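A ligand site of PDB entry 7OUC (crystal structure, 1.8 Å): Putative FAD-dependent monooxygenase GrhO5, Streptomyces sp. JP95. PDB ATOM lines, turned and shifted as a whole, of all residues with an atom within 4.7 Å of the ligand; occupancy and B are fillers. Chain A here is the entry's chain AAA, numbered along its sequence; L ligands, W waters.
Water W15 lies within hydrogen-bond range of O10 of the ligand (2.5 Å) and N of Ala 310 (3.0 Å).
Water W2 lies within hydrogen-bond range of an oxygen (O7) of the ligand (2.6 Å), the backbone carbonyl oxygen (O) of Gly 307 (2.8 Å), the backbone NH (N) of Ala 310 (2.8 Å) and the backbone NH (N) of Gly 309 (3.2 Å).
Water W12 lies within hydrogen-bond range of an oxygen (O2) of the ligand and the guanidinium group of Arg 41.
Water W13 lies within hydrogen-bond range of OD2 of Asp 297 (2.7 Å) and O1 of the ligand (2.7 Å).
Water W5 bridges an oxygen (O8) of the ligand (3.2 Å) and the backbone carbonyl oxygen of Arg 41 (3.3 Å).
Water W10 lies within hydrogen-bond range of NE2 of His 33, NH2 of Arg 32 and O6 of the ligand.
NE1 of Trp 277 sits close to N9 of the ligand (3.3 Å).
Residues that only touch the ligand: Val 7 (3.7 Å), Gly 8 (3.4 Å), Val 30 (3.8 Å), Arg 41 (3.5 Å), Ala 42 (3.8 Å), Ala 133 (3.6 Å), Glu 134 (3.6 Å), Ala 167 (3.4 Å), Asp 168 (3.3 Å), Gly 169 (3.2 Å), Pro 170 (3.3 Å), Ser 193 (3.4 Å), Phe 275 (3.7 Å), Pro 276 (3.9 Å), Gly 296 (3.3 Å), Pro 304 (3.7 Å), Gly 307 (3.7 Å) and Ala 310 (3.9 Å).
Hydrophobic or aromatic side chains that line the ligand: Val 7, Leu 11, Val 12, His 33, Ala 42, Leu 135, Pro 170, Phe 275, Trp 277 and Pro 304.
28 residues have an atom within 4 Å of the ligand: Val 7, Gly 8, Ser 10, Leu 11, Val 12, Val 30, Glu 31, Arg 32, His 33, Arg 41, Ala 42, Gln 111, Ala 133, Glu 134, Leu 135, Ala 167, Asp 168, Gly 169, Pro 170, Ser 193, Phe 275, Pro 276, Trp 277, Gly 296, Asp 297, Pro 304, Gly 307 and Ala 310.
The nearest printed residue that does not touch the ligand is Ala 295 (4.1 Å).
The backbone carbonyl oxygen of Val 7 is in hydrogen-bond range of the backbone NH of Asp 168.
The backbone NH (N) of Ser 193 sits at hydrogen-bond distance from the backbone carbonyl oxygen (O) of Phe 275 (2.8 Å).
OG of Ser 10 is in hydrogen-bond range of NH1 of Arg 41 (3.1 Å).
OE2 of Glu 31 is in hydrogen-bond range of N of His 33, 2.9 Å away.
N of Gly 8 is in hydrogen-bond range of O of Val 30, 2.9 Å away.
The side-chain amide oxygen of Gln 111 is in hydrogen-bond range of the side-chain hydroxyl of Ser 10, 3.5 Å away.
O of Ser 193 lies within hydrogen-bond range of NE2 of His 39, 3.2 Å away.
The backbone NH (N) of Arg 32 lies within hydrogen-bond range of the backbone carbonyl oxygen (O) of Ala 133, at 3.1 Å.
O10 of the ligand sits at hydrogen-bond distance from OD1 of Asp 297.
O2 of the ligand lies within hydrogen-bond range of OG of Ser 10, 2.8 Å away.
The backbone NH (N) of Val 12 lies within hydrogen-bond range of an oxygen (O13) of the ligand (3.0 Å).
OE1 of Gln 111 sits at hydrogen-bond distance from O11 of the ligand (2.7 Å).
N of Leu 11 is in hydrogen-bond range of O13 of the ligand (3.5 Å).
O of Leu 135 sits at hydrogen-bond distance from N3 of the ligand (2.9 Å).
The backbone NH (N) of Leu 135 lies within hydrogen-bond range of a nitrogen (N4) of the ligand, 2.9 Å away.
The backbone NH (N) of Asp 297 is in hydrogen-bond range of an oxygen (O14) of the ligand, at 2.8 Å.
NE2 of His 33 lies close to O6 of the ligand, 3.3 Å away.
The side-chain carboxylate (OE1) of Glu 31 is in hydrogen-bond range of an oxygen (O5) of the ligand.
A nitrogen (N5) of the ligand is in hydrogen-bond range of the backbone NH of Arg 32, at 3.1 Å.
The guanidinium group (NE) of Arg 32 lies within hydrogen-bond range of an oxygen (O6) of the ligand, at 3.0 Å.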
ATOM      1  N   VAL A   7      23.911  21.667  -0.941  1.00  0.00           N
ATOM      2  CA  VAL A   7      23.479  23.077  -0.767  1.00  0.00           C
ATOM      3  C   VAL A   7      22.310  23.025   0.196  1.00  0.00           C
ATOM      4  O   VAL A   7      21.309  22.398  -0.161  1.00  0.00           O
ATOM      5  CB  VAL A   7      23.083  23.705  -2.107  1.00  0.00           C
ATOM      6  CG1 VAL A   7      22.822  25.188  -1.974  1.00  0.00           C
ATOM      7  CG2 VAL A   7      24.146  23.396  -3.143  1.00  0.00           C
ATOM      8  N   GLY A   8      22.492  23.631   1.358  1.00  0.00           N
ATOM      9  CA  GLY A   8      21.472  23.726   2.419  1.00  0.00           C
ATOM     10  C   GLY A   8      21.890  23.003   3.656  1.00  0.00           C
ATOM     11  O   GLY A   8      22.165  21.782   3.532  1.00  0.00           O
ATOM     12  N   GLY A   9      21.927  23.708   4.791  1.00  0.00           N
ATOM     13  CA  GLY A   9      22.332  23.194   6.115  1.00  0.00           C
ATOM     14  C   GLY A   9      21.141  23.226   7.053  1.00  0.00           C
ATOM     15  O   GLY A   9      21.312  23.503   8.241  1.00  0.00           O
ATOM     16  N   SER A  10      19.965  22.939   6.513  1.00  0.00           N
ATOM     17  CA  SER A  10      18.765  22.677   7.310  1.00  0.00           C
ATOM     18  C   SER A  10      18.590  21.163   7.408  1.00  0.00           C
ATOM     19  O   SER A  10      19.545  20.442   7.228  1.00  0.00           O
ATOM     20  CB  SER A  10      17.603  23.361   6.734  1.00  0.00           C
ATOM     21  OG  SER A  10      16.514  23.274   7.595  1.00  0.00           O
ATOM     22  N   LEU A  11      17.435  20.720   7.833  1.00  0.00           N
ATOM     23  CA  LEU A  11      17.189  19.305   8.139  1.00  0.00           C
ATOM     24  C   LEU A  11      17.630  18.363   6.999  1.00  0.00           C
ATOM     25  O   LEU A  11      18.265  17.339   7.306  1.00  0.00           O
ATOM     26  CB  LEU A  11      15.702  19.163   8.398  1.00  0.00           C
ATOM     27  CG  LEU A  11      15.267  17.781   8.841  1.00  0.00           C
ATOM     28  CD1 LEU A  11      15.926  17.438  10.168  1.00  0.00           C
ATOM     29  CD2 LEU A  11      13.750  17.724   8.957  1.00  0.00           C
ATOM     30  N   VAL A  12      17.265  18.631   5.743  1.00  0.00           N
ATOM     31  CA  VAL A  12      17.516  17.612   4.691  1.00  0.00           C
ATOM     32  C   VAL A  12      18.990  17.646   4.301  1.00  0.00           C
ATOM     33  O   VAL A  12      19.573  16.569   4.100  1.00  0.00           O
ATOM     34  CB  VAL A  12      16.548  17.777   3.509  1.00  0.00           C
ATOM     35  CG1 VAL A  12      16.950  16.935   2.344  1.00  0.00           C
ATOM     36  CG2 VAL A  12      15.106  17.502   3.956  1.00  0.00           C
ATOM     37  N   GLY A  13      19.563  18.822   4.179  1.00  0.00           N
ATOM     38  CA  GLY A  13      20.997  18.948   3.842  1.00  0.00           C
ATOM     39  C   GLY A  13      21.850  18.284   4.895  1.00  0.00           C
ATOM     40  O   GLY A  13      22.745  17.481   4.554  1.00  0.00           O
ATOM     41  N   VAL A  30      27.313  23.481   2.006  1.00  0.00           N
ATOM     42  CA  VAL A  30      27.315  24.953   2.104  1.00  0.00           C
ATOM     43  C   VAL A  30      25.933  25.366   2.600  1.00  0.00           C
ATOM     44  O   VAL A  30      24.973  24.904   2.075  1.00  0.00           O
ATOM     45  CB  VAL A  30      27.754  25.623   0.781  1.00  0.00           C
ATOM     46  CG1 VAL A  30      29.193  25.300   0.467  1.00  0.00           C
ATOM     47  CG2 VAL A  30      26.853  25.280  -0.396  1.00  0.00           C
ATOM     48  N   GLU A  31      25.883  26.252   3.577  1.00  0.00           N
ATOM     49  CA  GLU A  31      24.651  26.846   4.104  1.00  0.00           C
ATOM     50  C   GLU A  31      24.903  28.348   4.200  1.00  0.00           C
ATOM     51  O   GLU A  31      25.875  28.703   4.864  1.00  0.00           O
ATOM     52  CB  GLU A  31      24.340  26.277   5.488  1.00  0.00           C
ATOM     53  CG  GLU A  31      23.283  27.053   6.279  1.00  0.00           C
ATOM     54  CD  GLU A  31      21.970  27.316   5.547  1.00  0.00           C
ATOM     55  OE1 GLU A  31      21.365  26.340   5.075  1.00  0.00           O
ATOM     56  OE2 GLU A  31      21.567  28.506   5.451  1.00  0.00           O
ATOM     57  N   ARG A  32      24.077  29.160   3.567  1.00  0.00           N
ATOM     58  CA  ARG A  32      24.288  30.621   3.531  1.00  0.00           C
ATOM     59  C   ARG A  32      24.204  31.221   4.947  1.00  0.00           C
ATOM     60  O   ARG A  32      24.922  32.207   5.207  1.00  0.00           O
ATOM     61  CB  ARG A  32      23.300  31.252   2.556  1.00  0.00           C
ATOM     62  CG  ARG A  32      21.845  31.206   3.016  1.00  0.00           C
ATOM     63  CD  ARG A  32      20.932  31.642   1.883  1.00  0.00           C
ATOM     64  NE  ARG A  32      19.574  31.337   2.236  1.00  0.00           N
ATOM     65  CZ  ARG A  32      18.548  31.480   1.421  1.00  0.00           C
ATOM     66  NH1 ARG A  32      18.750  31.980   0.207  1.00  0.00           N
ATOM     67  NH2 ARG A  32      17.330  31.137   1.819  1.00  0.00           N
ATOM     68  N   HIS A  33      23.326  30.725   5.818  1.00  0.00           N
ATOM     69  CA  HIS A  33      23.155  31.282   7.185  1.00  0.00           C
ATOM     70  C   HIS A  33      24.358  30.879   8.016  1.00  0.00           C
ATOM     71  O   HIS A  33      25.028  29.881   7.734  1.00  0.00           O
ATOM     72  CB  HIS A  33      21.816  30.914   7.857  1.00  0.00           C
ATOM     73  CG  HIS A  33      20.635  31.427   7.114  1.00  0.00           C
ATOM     74  ND1 HIS A  33      20.521  32.775   6.745  1.00  0.00           N
ATOM     75  CD2 HIS A  33      19.549  30.795   6.625  1.00  0.00           C
ATOM     76  CE1 HIS A  33      19.406  32.943   6.052  1.00  0.00           C
ATOM     77  NE2 HIS A  33      18.787  31.738   5.954  1.00  0.00           N
ATOM     78  N   HIS A  39      14.613  28.445  14.862  1.00  0.00           N
ATOM     79  CA  HIS A  39      13.140  28.290  14.745  1.00  0.00           C
ATOM     80  C   HIS A  39      12.754  26.828  14.929  1.00  0.00           C
ATOM     81  O   HIS A  39      13.447  25.927  14.438  1.00  0.00           O
ATOM     82  CB  HIS A  39      12.669  28.879  13.421  1.00  0.00           C
ATOM     83  CG  HIS A  39      12.796  30.353  13.367  1.00  0.00           C
ATOM     84  ND1 HIS A  39      14.030  30.982  13.305  1.00  0.00           N
ATOM     85  CD2 HIS A  39      11.867  31.306  13.359  1.00  0.00           C
ATOM     86  CE1 HIS A  39      13.842  32.277  13.302  1.00  0.00           C
ATOM     87  NE2 HIS A  39      12.543  32.498  13.282  1.00  0.00           N
ATOM     88  N   ARG A  41      10.146  25.160  13.838  1.00  0.00           N
ATOM     89  CA  ARG A  41       9.700  24.659  12.525  1.00  0.00           C
ATOM     90  C   ARG A  41       8.965  23.320  12.685  1.00  0.00           C
ATOM     91  O   ARG A  41       8.006  23.264  13.436  1.00  0.00           O
ATOM     92  CB  ARG A  41      10.935  24.610  11.615  1.00  0.00           C
ATOM     93  CG  ARG A  41      11.486  25.984  11.333  1.00  0.00           C
ATOM     94  CD  ARG A  41      12.844  25.995  10.665  1.00  0.00           C
ATOM     95  NE  ARG A  41      13.834  25.566  11.627  1.00  0.00           N
ATOM     96  CZ  ARG A  41      14.976  24.951  11.346  1.00  0.00           C
ATOM     97  NH1 ARG A  41      15.325  24.729  10.084  1.00  0.00           N
ATOM     98  NH2 ARG A  41      15.769  24.589  12.320  1.00  0.00           N
ATOM     99  N   ALA A  42       9.375  22.261  12.000  1.00  0.00           N
ATOM    100  CA  ALA A  42       8.689  20.949  12.111  1.00  0.00           C
ATOM    101  C   ALA A  42       9.041  20.267  13.415  1.00  0.00           C
ATOM    102  O   ALA A  42      10.239  20.173  13.727  1.00  0.00           O
ATOM    103  CB  ALA A  42       9.017  20.042  10.952  1.00  0.00           C
ATOM    104  N   GLN A 111      12.859  21.175  15.359  1.00  0.00           N
ATOM    105  CA  GLN A 111      13.900  21.094  14.342  1.00  0.00           C
ATOM    106  C   GLN A 111      15.166  21.773  14.837  1.00  0.00           C
ATOM    107  O   GLN A 111      16.255  21.312  14.507  1.00  0.00           O
ATOM    108  CB  GLN A 111      13.333  21.714  13.068  1.00  0.00           C
ATOM    109  CG  GLN A 111      13.915  21.117  11.849  1.00  0.00           C
ATOM    110  CD  GLN A 111      13.320  21.628  10.561  1.00  0.00           C
ATOM    111  OE1 GLN A 111      14.068  21.978   9.668  1.00  0.00           O
ATOM    112  NE2 GLN A 111      12.028  21.670  10.477  1.00  0.00           N
ATOM    113  N   ALA A 133      28.222  30.259   3.912  1.00  0.00           N
ATOM    114  CA  ALA A 133      28.706  29.987   2.534  1.00  0.00           C
ATOM    115  C   ALA A 133      27.496  29.845   1.601  1.00  0.00           C
ATOM    116  O   ALA A 133      26.648  28.959   1.818  1.00  0.00           O
ATOM    117  CB  ALA A 133      29.607  28.787   2.530  1.00  0.00           C
ATOM    118  N   GLU A 134      27.424  30.691   0.573  1.00  0.00           N
ATOM    119  CA  GLU A 134      26.270  30.800  -0.339  1.00  0.00           C
ATOM    120  C   GLU A 134      26.616  30.176  -1.696  1.00  0.00           C
ATOM    121  O   GLU A 134      27.639  30.581  -2.288  1.00  0.00           O
ATOM    122  CB  GLU A 134      25.925  32.268  -0.502  1.00  0.00           C
ATOM    123  CG  GLU A 134      24.602  32.516  -1.197  1.00  0.00           C
ATOM    124  CD  GLU A 134      24.359  33.990  -1.470  1.00  0.00           C
ATOM    125  OE1 GLU A 134      25.348  34.783  -1.477  1.00  0.00           O
ATOM    126  OE2 GLU A 134      23.190  34.350  -1.719  1.00  0.00           O
ATOM    127  N   LEU A 135      25.826  29.214  -2.157  1.00  0.00           N
ATOM    128  CA  LEU A 135      25.906  28.773  -3.573  1.00  0.00           C
ATOM    129  C   LEU A 135      25.395  29.932  -4.434  1.00  0.00           C
ATOM    130  O   LEU A 135      24.230  30.319  -4.250  1.00  0.00           O
ATOM    131  CB  LEU A 135      25.052  27.533  -3.830  1.00  0.00           C
ATOM    132  CG  LEU A 135      25.088  27.144  -5.303  1.00  0.00           C
ATOM    133  CD1 LEU A 135      26.293  26.277  -5.560  1.00  0.00           C
ATOM    134  CD2 LEU A 135      23.803  26.468  -5.767  1.00  0.00           C
ATOM    135  N   ALA A 167      19.404  20.700  -1.371  1.00  0.00           N
ATOM    136  CA  ALA A 167      18.537  20.696  -0.164  1.00  0.00           C
ATOM    137  C   ALA A 167      18.342  22.163   0.266  1.00  0.00           C
ATOM    138  O   ALA A 167      18.394  22.432   1.449  1.00  0.00           O
ATOM    139  CB  ALA A 167      19.188  19.878   0.902  1.00  0.00           C
ATOM    140  N   ASP A 168      18.065  23.021  -0.704  1.00  0.00           N
ATOM    141  CA  ASP A 168      18.125  24.507  -0.541  1.00  0.00           C
ATOM    142  C   ASP A 168      16.715  25.087  -0.416  1.00  0.00           C
ATOM    143  O   ASP A 168      16.547  26.313  -0.476  1.00  0.00           O
ATOM    144  CB  ASP A 168      18.978  25.126  -1.650  1.00  0.00           C
ATOM    145  CG  ASP A 168      18.566  24.840  -3.083  1.00  0.00           C
ATOM    146  OD1 ASP A 168      17.942  23.764  -3.359  1.00  0.00           O
ATOM    147  OD2 ASP A 168      18.913  25.687  -3.951  1.00  0.00           O
ATOM    148  N   GLY A 169      15.731  24.246  -0.128  1.00  0.00           N
ATOM    149  CA  GLY A 169      14.422  24.698   0.388  1.00  0.00           C
ATOM    150  C   GLY A 169      13.450  25.081  -0.727  1.00  0.00           C
ATOM    151  O   GLY A 169      13.712  24.885  -1.904  1.00  0.00           O
ATOM    152  N   PRO A 170      12.250  25.582  -0.370  1.00  0.00           N
ATOM    153  CA  PRO A 170      11.168  25.777  -1.324  1.00  0.00           C
ATOM    154  C   PRO A 170      11.474  26.641  -2.550  1.00  0.00           C
ATOM    155  O   PRO A 170      10.982  26.331  -3.593  1.00  0.00           O
ATOM    156  CB  PRO A 170      10.074  26.482  -0.527  1.00  0.00           C
ATOM    157  CG  PRO A 170      10.359  26.083   0.883  1.00  0.00           C
ATOM    158  CD  PRO A 170      11.874  25.986   0.986  1.00  0.00           C
ATOM    159  N   THR A 173      17.121  27.887  -5.691  1.00  0.00           N
ATOM    160  CA  THR A 173      17.709  28.468  -6.933  1.00  0.00           C
ATOM    161  C   THR A 173      18.315  27.333  -7.783  1.00  0.00           C
ATOM    162  O   THR A 173      18.461  27.548  -8.988  1.00  0.00           O
ATOM    163  CB  THR A 173      18.708  29.590  -6.638  1.00  0.00           C
ATOM    164  OG1 THR A 173      19.782  29.030  -5.896  1.00  0.00           O
ATOM    165  CG2 THR A 173      18.061  30.757  -5.909  1.00  0.00           C
ATOM    166  N   SER A 193       7.630  33.373  10.730  1.00  0.00           N
ATOM    167  CA  SER A 193       8.050  32.792  12.010  1.00  0.00           C
ATOM    168  C   SER A 193       8.982  33.779  12.689  1.00  0.00           C
ATOM    169  O   SER A 193      10.015  34.121  12.067  1.00  0.00           O
ATOM    170  CB  SER A 193       8.728  31.448  11.779  1.00  0.00           C
ATOM    171  OG  SER A 193       9.131  30.891  13.017  1.00  0.00           O
ATOM    172  N   PHE A 275      11.708  34.520   9.835  1.00  0.00           N
ATOM    173  CA  PHE A 275      11.798  33.862   8.509  1.00  0.00           C
ATOM    174  C   PHE A 275      10.426  33.695   7.903  1.00  0.00           C
ATOM    175  O   PHE A 275       9.494  33.396   8.617  1.00  0.00           O
ATOM    176  CB  PHE A 275      12.393  32.458   8.603  1.00  0.00           C
ATOM    177  CG  PHE A 275      13.867  32.360   8.882  1.00  0.00           C
ATOM    178  CD1 PHE A 275      14.382  32.674  10.133  1.00  0.00           C
ATOM    179  CD2 PHE A 275      14.712  31.747   7.973  1.00  0.00           C
ATOM    180  CE1 PHE A 275      15.731  32.571  10.396  1.00  0.00           C
ATOM    181  CE2 PHE A 275      16.055  31.568   8.256  1.00  0.00           C
ATOM    182  CZ  PHE A 275      16.560  31.980   9.470  1.00  0.00           C
ATOM    183  N   PRO A 276      10.316  33.841   6.568  1.00  0.00           N
ATOM    184  CA  PRO A 276       9.073  33.580   5.859  1.00  0.00           C
ATOM    185  C   PRO A 276       8.897  32.063   5.788  1.00  0.00           C
ATOM    186  O   PRO A 276       9.874  31.295   5.771  1.00  0.00           O
ATOM    187  CB  PRO A 276       9.297  34.235   4.503  1.00  0.00           C
ATOM    188  CG  PRO A 276      10.796  34.121   4.281  1.00  0.00           C
ATOM    189  CD  PRO A 276      11.409  34.209   5.649  1.00  0.00           C
ATOM    190  N   TRP A 277       7.657  31.668   5.835  1.00  0.00           N
ATOM    191  CA  TRP A 277       7.282  30.268   5.566  1.00  0.00           C
ATOM    192  C   TRP A 277       5.878  30.237   4.961  1.00  0.00           C
ATOM    193  O   TRP A 277       4.960  30.884   5.506  1.00  0.00           O
ATOM    194  CB  TRP A 277       7.370  29.460   6.846  1.00  0.00           C
ATOM    195  CG  TRP A 277       6.951  28.064   6.607  1.00  0.00           C
ATOM    196  CD1 TRP A 277       7.484  27.139   5.760  1.00  0.00           C
ATOM    197  CD2 TRP A 277       5.884  27.444   7.298  1.00  0.00           C
ATOM    198  NE1 TRP A 277       6.785  25.971   5.870  1.00  0.00           N
ATOM    199  CE2 TRP A 277       5.814  26.127   6.816  1.00  0.00           C
ATOM    200  CE3 TRP A 277       5.044  27.882   8.326  1.00  0.00           C
ATOM    201  CZ2 TRP A 277       4.887  25.233   7.304  1.00  0.00           C
ATOM    202  CZ3 TRP A 277       4.110  26.998   8.786  1.00  0.00           C
ATOM    203  CH2 TRP A 277       4.033  25.705   8.281  1.00  0.00           C
ATOM    204  N   ALA A 295      16.173  17.362  -3.220  1.00  0.00           N
ATOM    205  CA  ALA A 295      15.621  16.664  -2.027  1.00  0.00           C
ATOM    206  C   ALA A 295      14.933  17.659  -1.113  1.00  0.00           C
ATOM    207  O   ALA A 295      15.223  18.881  -1.174  1.00  0.00           O
ATOM    208  CB  ALA A 295      16.678  15.909  -1.294  1.00  0.00           C
ATOM    209  N   GLY A 296      14.037  17.141  -0.283  1.00  0.00           N
ATOM    210  CA  GLY A 296      13.406  17.951   0.755  1.00  0.00           C
ATOM    211  C   GLY A 296      12.450  18.950   0.161  1.00  0.00           C
ATOM    212  O   GLY A 296      11.775  18.632  -0.835  1.00  0.00           O
ATOM    213  N   ASP A 297      12.406  20.143   0.761  1.00  0.00           N
ATOM    214  CA  ASP A 297      11.434  21.179   0.361  1.00  0.00           C
ATOM    215  C   ASP A 297      11.658  21.632  -1.080  1.00  0.00           C
ATOM    216  O   ASP A 297      10.686  22.064  -1.698  1.00  0.00           O
ATOM    217  CB  ASP A 297      11.429  22.329   1.345  1.00  0.00           C
ATOM    218  CG  ASP A 297      10.553  22.048   2.561  1.00  0.00           C
ATOM    219  OD1 ASP A 297      10.273  20.836   2.832  1.00  0.00           O
ATOM    220  OD2 ASP A 297      10.239  23.056   3.269  1.00  0.00           O
ATOM    221  N   ALA A 298      12.890  21.589  -1.578  1.00  0.00           N
ATOM    222  CA  ALA A 298      13.210  21.937  -2.980  1.00  0.00           C
ATOM    223  C   ALA A 298      12.468  20.985  -3.930  1.00  0.00           C
ATOM    224  O   ALA A 298      12.093  21.406  -5.034  1.00  0.00           O
ATOM    225  CB  ALA A 298      14.715  21.897  -3.160  1.00  0.00           C
ATOM    226  N   PRO A 304       1.706  21.722   6.174  1.00  0.00           N
ATOM    227  CA  PRO A 304       2.286  21.305   7.454  1.00  0.00           C
ATOM    228  C   PRO A 304       1.435  20.388   8.335  1.00  0.00           C
ATOM    229  O   PRO A 304       1.988  19.887   9.283  1.00  0.00           O
ATOM    230  CB  PRO A 304       2.463  22.651   8.179  1.00  0.00           C
ATOM    231  CG  PRO A 304       1.354  23.522   7.612  1.00  0.00           C
ATOM    232  CD  PRO A 304       1.411  23.161   6.126  1.00  0.00           C
ATOM    233  N   GLY A 307       2.805  17.250   9.903  1.00  0.00           N
ATOM    234  CA  GLY A 307       4.265  17.425   9.736  1.00  0.00           C
ATOM    235  C   GLY A 307       4.872  16.369   8.817  1.00  0.00           C
ATOM    236  O   GLY A 307       5.951  15.833   9.166  1.00  0.00           O
ATOM    237  N   GLY A 309       6.212  16.863   5.797  1.00  0.00           N
ATOM    238  CA  GLY A 309       7.265  17.454   4.945  1.00  0.00           C
ATOM    239  C   GLY A 309       8.654  17.090   5.455  1.00  0.00           C
ATOM    240  O   GLY A 309       9.491  16.570   4.657  1.00  0.00           O
ATOM    241  N   ALA A 310       8.924  17.357   6.752  1.00  0.00           N
ATOM    242  CA  ALA A 310      10.250  17.155   7.348  1.00  0.00           C
ATOM    243  C   ALA A 310      10.576  15.663   7.301  1.00  0.00           C
ATOM    244  O   ALA A 310      11.721  15.275   6.979  1.00  0.00           O
ATOM    245  CB  ALA A 310      10.282  17.707   8.740  1.00  0.00           C
HETATM  246  P1  LIG L   1      14.733  24.176   4.280  1.00  0.00           P
HETATM  247  O1  LIG L   1      13.909  25.121   3.500  1.00  0.00           O
HETATM  248  O2  LIG L   1      14.445  23.745   5.701  1.00  0.00           O
HETATM  249  O3  LIG L   1      16.257  24.634   4.283  1.00  0.00           O
HETATM  250  C1  LIG L   1      16.920  25.030   3.073  1.00  0.00           C
HETATM  251  C2  LIG L   1      18.248  25.618   3.493  1.00  0.00           C
HETATM  252  O4  LIG L   1      18.971  25.987   2.295  1.00  0.00           O
HETATM  253  C3  LIG L   1      18.181  26.889   4.377  1.00  0.00           C
HETATM  254  O5  LIG L   1      18.909  26.747   5.601  1.00  0.00           O
HETATM  255  C4  LIG L   1      18.681  27.996   3.434  1.00  0.00           C
HETATM  256  O6  LIG L   1      19.310  29.067   4.113  1.00  0.00           O
HETATM  257  C5  LIG L   1      19.638  27.210   2.546  1.00  0.00           C
HETATM  258  N1  LIG L   1      19.953  27.814   1.287  1.00  0.00           N
HETATM  259  C6  LIG L   1      19.080  28.257   0.352  1.00  0.00           C
HETATM  260  N2  LIG L   1      19.681  28.742  -0.722  1.00  0.00           N
HETATM  261  C7  LIG L   1      21.033  28.586  -0.455  1.00  0.00           C
HETATM  262  C8  LIG L   1      22.176  28.910  -1.201  1.00  0.00           C
HETATM  263  N3  LIG L   1      22.123  29.488  -2.395  1.00  0.00           N
HETATM  264  N4  LIG L   1      23.379  28.612  -0.658  1.00  0.00           N
HETATM  265  C9  LIG L   1      23.394  28.061   0.562  1.00  0.00           C
HETATM  266  N5  LIG L   1      22.383  27.730   1.352  1.00  0.00           N
HETATM  267  C10 LIG L   1      21.207  28.014   0.768  1.00  0.00           C
HETATM  268  N6  LIG L   1       7.280  22.368   8.328  1.00  0.00           N
HETATM  269  C11 LIG L   1       6.243  21.818   9.017  1.00  0.00           C
HETATM  270  O7  LIG L   1       5.849  20.677   8.786  1.00  0.00           O
HETATM  271  N7  LIG L   1       5.644  22.480  10.049  1.00  0.00           N
HETATM  272  C12 LIG L   1       5.977  23.763  10.400  1.00  0.00           C
HETATM  273  O8  LIG L   1       5.378  24.323  11.305  1.00  0.00           O
HETATM  274  C13 LIG L   1       7.015  24.379   9.698  1.00  0.00           C
HETATM  275  N8  LIG L   1       7.376  25.594  10.049  1.00  0.00           N
HETATM  276  C14 LIG L   1       8.392  26.183   9.336  1.00  0.00           C
HETATM  277  C15 LIG L   1       8.784  27.494   9.658  1.00  0.00           C
HETATM  278  C16 LIG L   1       9.808  28.116   8.996  1.00  0.00           C
HETATM  279  C17 LIG L   1      10.200  29.531   9.383  1.00  0.00           C
HETATM  280  C18 LIG L   1      10.469  27.454   7.950  1.00  0.00           C
HETATM  281  C19 LIG L   1      11.586  28.114   7.178  1.00  0.00           C
HETATM  282  C20 LIG L   1      10.090  26.169   7.620  1.00  0.00           C
HETATM  283  C21 LIG L   1       9.053  25.521   8.290  1.00  0.00           C
HETATM  284  N9  LIG L   1       8.672  24.210   7.987  1.00  0.00           N
HETATM  285  C22 LIG L   1       7.642  23.603   8.667  1.00  0.00           C
HETATM  286  C23 LIG L   1       9.327  23.473   6.899  1.00  0.00           C
HETATM  287  C24 LIG L   1      10.387  22.525   7.407  1.00  0.00           C
HETATM  288  O9  LIG L   1      11.258  23.265   8.247  1.00  0.00           O
HETATM  289  C25 LIG L   1      11.084  21.812   6.238  1.00  0.00           C
HETATM  290  O10 LIG L   1      10.168  20.905   5.765  1.00  0.00           O
HETATM  291  C26 LIG L   1      12.338  21.006   6.548  1.00  0.00           C
HETATM  292  O11 LIG L   1      13.320  21.842   7.129  1.00  0.00           O
HETATM  293  C27 LIG L   1      12.899  20.308   5.332  1.00  0.00           C
HETATM  294  O12 LIG L   1      13.277  21.298   4.372  1.00  0.00           O
HETATM  295  P2  LIG L   1      14.738  21.291   3.755  1.00  0.00           P
HETATM  296  O13 LIG L   1      15.773  21.047   4.792  1.00  0.00           O
HETATM  297  O14 LIG L   1      14.598  20.500   2.504  1.00  0.00           O
HETATM  298  O15 LIG L   1      14.827  22.844   3.418  1.00  0.00           O
HETATM  299  O   HOH W   1      14.465  27.659   3.313  1.00  0.00           O
HETATM  300  O   HOH W   2       6.980  18.327   8.590  1.00  0.00           O
HETATM  301  O   HOH W   3       4.840  19.267   6.190  1.00  0.00           O
HETATM  302  O   HOH W   4       3.618  20.941  11.328  1.00  0.00           O
HETATM  303  O   HOH W   5       6.855  26.374  13.238  1.00  0.00           O
HETATM  304  O   HOH W   6      18.912  28.222  -3.444  1.00  0.00           O
HETATM  305  O   HOH W   7      10.244  27.753   4.032  1.00  0.00           O
HETATM  306  O   HOH W   8      12.482  30.801   5.165  1.00  0.00           O
HETATM  307  O   HOH W   9      17.729  27.089   8.083  1.00  0.00           O
HETATM  308  O   HOH W  10      16.544  30.977   4.697  1.00  0.00           O
HETATM  309  O   HOH W  11      18.433  21.465   4.130  1.00  0.00           O
HETATM  310  O   HOH W  12      13.493  25.181   7.707  1.00  0.00           O
HETATM  311  O   HOH W  13      11.345  25.260   4.281  1.00  0.00           O
HETATM  312  O   HOH W  14      19.896  31.167  -3.406  1.00  0.00           O
HETATM  313  O   HOH W  15       7.891  20.217   6.677  1.00  0.00           O
HETATM  314  O   HOH W  16      15.283  21.303   0.075  1.00  0.00           O
